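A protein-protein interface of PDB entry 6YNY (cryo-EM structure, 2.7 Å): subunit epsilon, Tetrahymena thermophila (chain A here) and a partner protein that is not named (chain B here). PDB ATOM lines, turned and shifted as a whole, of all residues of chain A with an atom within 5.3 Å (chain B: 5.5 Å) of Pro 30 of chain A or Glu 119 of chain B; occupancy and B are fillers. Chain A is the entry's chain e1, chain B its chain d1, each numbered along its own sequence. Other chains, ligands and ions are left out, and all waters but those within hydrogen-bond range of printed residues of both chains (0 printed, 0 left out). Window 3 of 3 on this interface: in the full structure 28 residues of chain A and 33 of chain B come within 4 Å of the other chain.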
ATOM      1  N   ILE A  26     -27.263  14.433  15.785  1.00  0.00           N
ATOM      2  CA  ILE A  26     -26.191  14.593  16.765  1.00  0.00           C
ATOM      3  C   ILE A  26     -26.180  13.416  17.732  1.00  0.00           C
ATOM      4  O   ILE A  26     -25.115  12.930  18.129  1.00  0.00           O
ATOM      5  CB  ILE A  26     -26.328  15.935  17.509  1.00  0.00           C
ATOM      6  CG1 ILE A  26     -27.701  16.055  18.173  1.00  0.00           C
ATOM      7  CG2 ILE A  26     -26.089  17.101  16.564  1.00  0.00           C
ATOM      8  CD1 ILE A  26     -27.892  17.346  18.936  1.00  0.00           C
ATOM      9  N   GLY A  28     -27.285  10.384  17.051  1.00  0.00           N
ATOM     10  CA  GLY A  28     -26.881   9.186  16.332  1.00  0.00           C
ATOM     11  C   GLY A  28     -25.375   9.061  16.205  1.00  0.00           C
ATOM     12  O   GLY A  28     -24.826   7.960  16.287  1.00  0.00           O
ATOM     13  N   LEU A  29     -24.688  10.182  16.009  1.00  0.00           N
ATOM     14  CA  LEU A  29     -23.242  10.146  15.878  1.00  0.00           C
ATOM     15  C   LEU A  29     -22.596   9.819  17.223  1.00  0.00           C
ATOM     16  O   LEU A  29     -23.180  10.072  18.281  1.00  0.00           O
ATOM     17  CB  LEU A  29     -22.718  11.483  15.362  1.00  0.00           C
ATOM     18  CG  LEU A  29     -23.376  12.009  14.086  1.00  0.00           C
ATOM     19  CD1 LEU A  29     -22.527  13.108  13.473  1.00  0.00           C
ATOM     20  CD2 LEU A  29     -23.611  10.884  13.090  1.00  0.00           C
ATOM     21  N   PRO A  30     -21.391   9.252  17.212  1.00  0.00           N
ATOM     22  CA  PRO A  30     -20.727   8.920  18.475  1.00  0.00           C
ATOM     23  C   PRO A  30     -20.476  10.159  19.320  1.00  0.00           C
ATOM     24  O   PRO A  30     -20.436  11.289  18.829  1.00  0.00           O
ATOM     25  CB  PRO A  30     -19.412   8.269  18.029  1.00  0.00           C
ATOM     26  CG  PRO A  30     -19.197   8.750  16.634  1.00  0.00           C
ATOM     27  CD  PRO A  30     -20.561   8.903  16.046  1.00  0.00           C
ATOM     28  N   GLN A  31     -20.305   9.924  20.623  1.00  0.00           N
ATOM     29  CA  GLN A  31     -20.060  11.025  21.548  1.00  0.00           C
ATOM     30  C   GLN A  31     -18.838  11.837  21.144  1.00  0.00           C
ATOM     31  O   GLN A  31     -18.750  13.027  21.467  1.00  0.00           O
ATOM     32  CB  GLN A  31     -19.903  10.483  22.971  1.00  0.00           C
ATOM     33  CG  GLN A  31     -18.805   9.436  23.137  1.00  0.00           C
ATOM     34  CD  GLN A  31     -17.421  10.043  23.247  1.00  0.00           C
ATOM     35  OE1 GLN A  31     -17.268  11.200  23.633  1.00  0.00           O
ATOM     36  NE2 GLN A  31     -16.404   9.261  22.903  1.00  0.00           N
ATOM     37  N   ARG A  32     -17.887  11.217  20.441  1.00  0.00           N
ATOM     38  CA  ARG A  32     -16.718  11.952  19.970  1.00  0.00           C
ATOM     39  C   ARG A  32     -17.131  13.157  19.135  1.00  0.00           C
ATOM     40  O   ARG A  32     -16.593  14.257  19.306  1.00  0.00           O
ATOM     41  CB  ARG A  32     -15.812  11.024  19.163  1.00  0.00           C
ATOM     42  CG  ARG A  32     -14.611  11.707  18.532  1.00  0.00           C
ATOM     43  CD  ARG A  32     -13.707  10.696  17.847  1.00  0.00           C
ATOM     44  NE  ARG A  32     -14.438   9.870  16.890  1.00  0.00           N
ATOM     45  CZ  ARG A  32     -14.712  10.228  15.639  1.00  0.00           C
ATOM     46  NH1 ARG A  32     -14.321  11.407  15.176  1.00  0.00           N
ATOM     47  NH2 ARG A  32     -15.384   9.402  14.850  1.00  0.00           N
ATOM     48  N   VAL A  33     -18.086  12.966  18.226  1.00  0.00           N
ATOM     49  CA  VAL A  33     -18.540  14.070  17.390  1.00  0.00           C
ATOM     50  C   VAL A  33     -19.452  15.003  18.176  1.00  0.00           C
ATOM     51  O   VAL A  33     -19.506  16.206  17.896  1.00  0.00           O
ATOM     52  CB  VAL A  33     -19.243  13.528  16.134  1.00  0.00           C
ATOM     53  CG1 VAL A  33     -19.719  14.672  15.255  1.00  0.00           C
ATOM     54  CG2 VAL A  33     -18.312  12.600  15.364  1.00  0.00           C
ATOM     55  N   GLN A  34     -20.177  14.475  19.165  1.00  0.00           N
ATOM     56  CA  GLN A  34     -21.111  15.300  19.923  1.00  0.00           C
ATOM     57  C   GLN A  34     -20.384  16.396  20.691  1.00  0.00           C
ATOM     58  O   GLN A  34     -20.828  17.551  20.708  1.00  0.00           O
ATOM     59  CB  GLN A  34     -21.922  14.423  20.876  1.00  0.00           C
ATOM     60  CG  GLN A  34     -22.790  13.399  20.169  1.00  0.00           C
ATOM     61  CD  GLN A  34     -23.582  12.535  21.130  1.00  0.00           C
ATOM     62  OE1 GLN A  34     -23.483  12.690  22.347  1.00  0.00           O
ATOM     63  NE2 GLN A  34     -24.372  11.618  20.586  1.00  0.00           N
ATOM     64  N   PHE B 115     -16.617  10.274  10.356  1.00  0.00           N
ATOM     65  CA  PHE B 115     -16.795   9.046  11.117  1.00  0.00           C
ATOM     66  C   PHE B 115     -17.111   7.919  10.145  1.00  0.00           C
ATOM     67  O   PHE B 115     -17.417   8.149   8.973  1.00  0.00           O
ATOM     68  CB  PHE B 115     -17.902   9.192  12.165  1.00  0.00           C
ATOM     69  CG  PHE B 115     -19.228   9.591  11.590  1.00  0.00           C
ATOM     70  CD1 PHE B 115     -20.133   8.630  11.175  1.00  0.00           C
ATOM     71  CD2 PHE B 115     -19.571  10.925  11.466  1.00  0.00           C
ATOM     72  CE1 PHE B 115     -21.355   8.992  10.646  1.00  0.00           C
ATOM     73  CE2 PHE B 115     -20.793  11.294  10.938  1.00  0.00           C
ATOM     74  CZ  PHE B 115     -21.684  10.325  10.526  1.00  0.00           C
ATOM     75  N   ASP B 116     -17.032   6.692  10.650  1.00  0.00           N
ATOM     76  CA  ASP B 116     -17.283   5.507   9.845  1.00  0.00           C
ATOM     77  C   ASP B 116     -18.752   5.109   9.925  1.00  0.00           C
ATOM     78  O   ASP B 116     -19.464   5.447  10.873  1.00  0.00           O
ATOM     79  CB  ASP B 116     -16.404   4.344  10.309  1.00  0.00           C
ATOM     80  CG  ASP B 116     -14.925   4.660  10.222  1.00  0.00           C
ATOM     81  OD1 ASP B 116     -14.532   5.440   9.330  1.00  0.00           O
ATOM     82  OD2 ASP B 116     -14.153   4.126  11.046  1.00  0.00           O
ATOM     83  N   ARG B 117     -19.203   4.376   8.904  1.00  0.00           N
ATOM     84  CA  ARG B 117     -20.578   3.890   8.904  1.00  0.00           C
ATOM     85  C   ARG B 117     -20.829   2.927  10.055  1.00  0.00           C
ATOM     86  O   ARG B 117     -21.932   2.898  10.611  1.00  0.00           O
ATOM     87  CB  ARG B 117     -20.905   3.213   7.573  1.00  0.00           C
ATOM     88  CG  ARG B 117     -21.086   4.172   6.412  1.00  0.00           C
ATOM     89  CD  ARG B 117     -21.722   3.470   5.224  1.00  0.00           C
ATOM     90  NE  ARG B 117     -20.900   2.366   4.739  1.00  0.00           N
ATOM     91  CZ  ARG B 117     -21.279   1.510   3.794  1.00  0.00           C
ATOM     92  NH1 ARG B 117     -20.462   0.536   3.416  1.00  0.00           N
ATOM     93  NH2 ARG B 117     -22.473   1.623   3.230  1.00  0.00           N
ATOM     94  N   LYS B 118     -19.822   2.133  10.425  1.00  0.00           N
ATOM     95  CA  LYS B 118     -20.017   1.134  11.469  1.00  0.00           C
ATOM     96  C   LYS B 118     -20.374   1.770  12.802  1.00  0.00           C
ATOM     97  O   LYS B 118     -20.998   1.113  13.644  1.00  0.00           O
ATOM     98  CB  LYS B 118     -18.756   0.281  11.624  1.00  0.00           C
ATOM     99  CG  LYS B 118     -18.135  -0.181  10.310  1.00  0.00           C
ATOM    100  CD  LYS B 118     -19.161  -0.813   9.381  1.00  0.00           C
ATOM    101  CE  LYS B 118     -18.514  -1.277   8.087  1.00  0.00           C
ATOM    102  NZ  LYS B 118     -19.518  -1.752   7.095  1.00  0.00           N
ATOM    103  N   GLU B 119     -19.997   3.030  13.014  1.00  0.00           N
ATOM    104  CA  GLU B 119     -20.336   3.762  14.227  1.00  0.00           C
ATOM    105  C   GLU B 119     -21.554   4.656  14.030  1.00  0.00           C
ATOM    106  O   GLU B 119     -21.727   5.634  14.765  1.00  0.00           O
ATOM    107  CB  GLU B 119     -19.135   4.591  14.685  1.00  0.00           C
ATOM    108  CG  GLU B 119     -19.164   4.974  16.155  1.00  0.00           C
ATOM    109  CD  GLU B 119     -17.851   5.566  16.628  1.00  0.00           C
ATOM    110  OE1 GLU B 119     -17.008   5.903  15.771  1.00  0.00           O
ATOM    111  OE2 GLU B 119     -17.660   5.691  17.856  1.00  0.00           O
ATOM    112  N   VAL B 120     -22.400   4.339  13.047  1.00  0.00           N
ATOM    113  CA  VAL B 120     -23.555   5.183  12.757  1.00  0.00           C
ATOM    114  C   VAL B 120     -24.510   5.210  13.942  1.00  0.00           C
ATOM    115  O   VAL B 120     -25.040   6.266  14.307  1.00  0.00           O
ATOM    116  CB  VAL B 120     -24.259   4.703  11.473  1.00  0.00           C
ATOM    117  CG1 VAL B 120     -24.786   3.281  11.642  1.00  0.00           C
ATOM    118  CG2 VAL B 120     -25.389   5.653  11.101  1.00  0.00           C
ATOM    119  N   ARG B 121     -24.746   4.054  14.561  1.00  0.00           N
ATOM    120  CA  ARG B 121     -25.688   3.938  15.670  1.00  0.00           C
ATOM    121  C   ARG B 121     -27.061   4.469  15.254  1.00  0.00           C
ATOM    122  O   ARG B 121     -27.618   5.389  15.856  1.00  0.00           O
ATOM    123  CB  ARG B 121     -25.163   4.669  16.909  1.00  0.00           C
ATOM    124  CG  ARG B 121     -25.951   4.382  18.174  1.00  0.00           C
ATOM    125  CD  ARG B 121     -25.561   5.320  19.310  1.00  0.00           C
ATOM    126  NE  ARG B 121     -24.149   5.202  19.670  1.00  0.00           N
ATOM    127  CZ  ARG B 121     -23.169   5.934  19.147  1.00  0.00           C
ATOM    128  NH1 ARG B 121     -21.919   5.744  19.548  1.00  0.00           N
ATOM    129  NH2 ARG B 121     -23.427   6.856  18.227  1.00  0.00           N
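Printed residues of chain B that touch a printed residue of chain A: Phe 115, Glu 119, Val 120 and Arg 121. Hydrophobic or aromatic side chains of chain B that line the printed part of chain A: Phe 115. Hydrophobic or aromatic side chains of chain A that line the printed part of chain B: Leu 29 and Pro 30. Among the printed residues, 8 pairs touch across the chains. Among the printed residues, Asp or Glu carboxylates within 4 Å of a Lys or Arg side-chain nitrogen of the other chain: Arg 32 of chain A with Glu 119 of chain B.
Among the printed residues, pairs that only touch across the chains: Pro 30 of chain A with Glu 119 of chain B (3.1 Å), Leu 29 of chain A with Phe 115 of chain B (3.3 Å) and Arg 32 of chain A with Phe 115 of chain B (3.7 Å).
The backbone carbonyl oxygen (O) of Leu 29 of chain A sits at hydrogen-bond distance from the side-chain amide nitrogen (NE2) of Gln 34 of chain A.
Glu 119 of chain B touches two residues of chain A. Printed residues of chain B within 4 Å of Arg 32 of chain A: Phe 115 (3.7 Å) and Glu 119 (3.97 Å). Of the printed residues of chain B, Gly 28 of chain A touches Val 120 and Arg 121. Printed residues of chain A within 4 Å of Val 120 of chain B: Gly 28. Of the printed residues of chain B, Leu 29 of chain A touches Phe 115 (3.3 Å) and Arg 121 (3.2 Å). Arg 117 of chain B touches none of the printed residues of chain A. The nearest residue of chain B that does not touch Pro 30 of chain A is Phe 115 of chain B (4.7 Å). The nearest residue of chain A that does not touch Glu 119 of chain B is Gly 28 of chain A (4.2 Å).
NH2 of Arg 32 of chain A lies within salt-bridge range of OE1 of Glu 119 of chain B (3.97 Å). The backbone carbonyl oxygen (O) of Gly 28 of chain A lies within hydrogen-bond range of the guanidinium group (NH2) of Arg 121 of chain B (2.6 Å). The guanidinium group of Arg 121 of chain B lies within hydrogen-bond range of the backbone carbonyl oxygen of Leu 29 of chain A, 3.2 Å away. The backbone nitrogen of Pro 30 of chain A sits close to the guanidinium group of Arg 121 of chain B (3.3 Å). The backbone carbonyl oxygen of Val 120 of chain B sits close to the backbone carbonyl oxygen of Gly 28 of chain A, 2.6 Å away.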
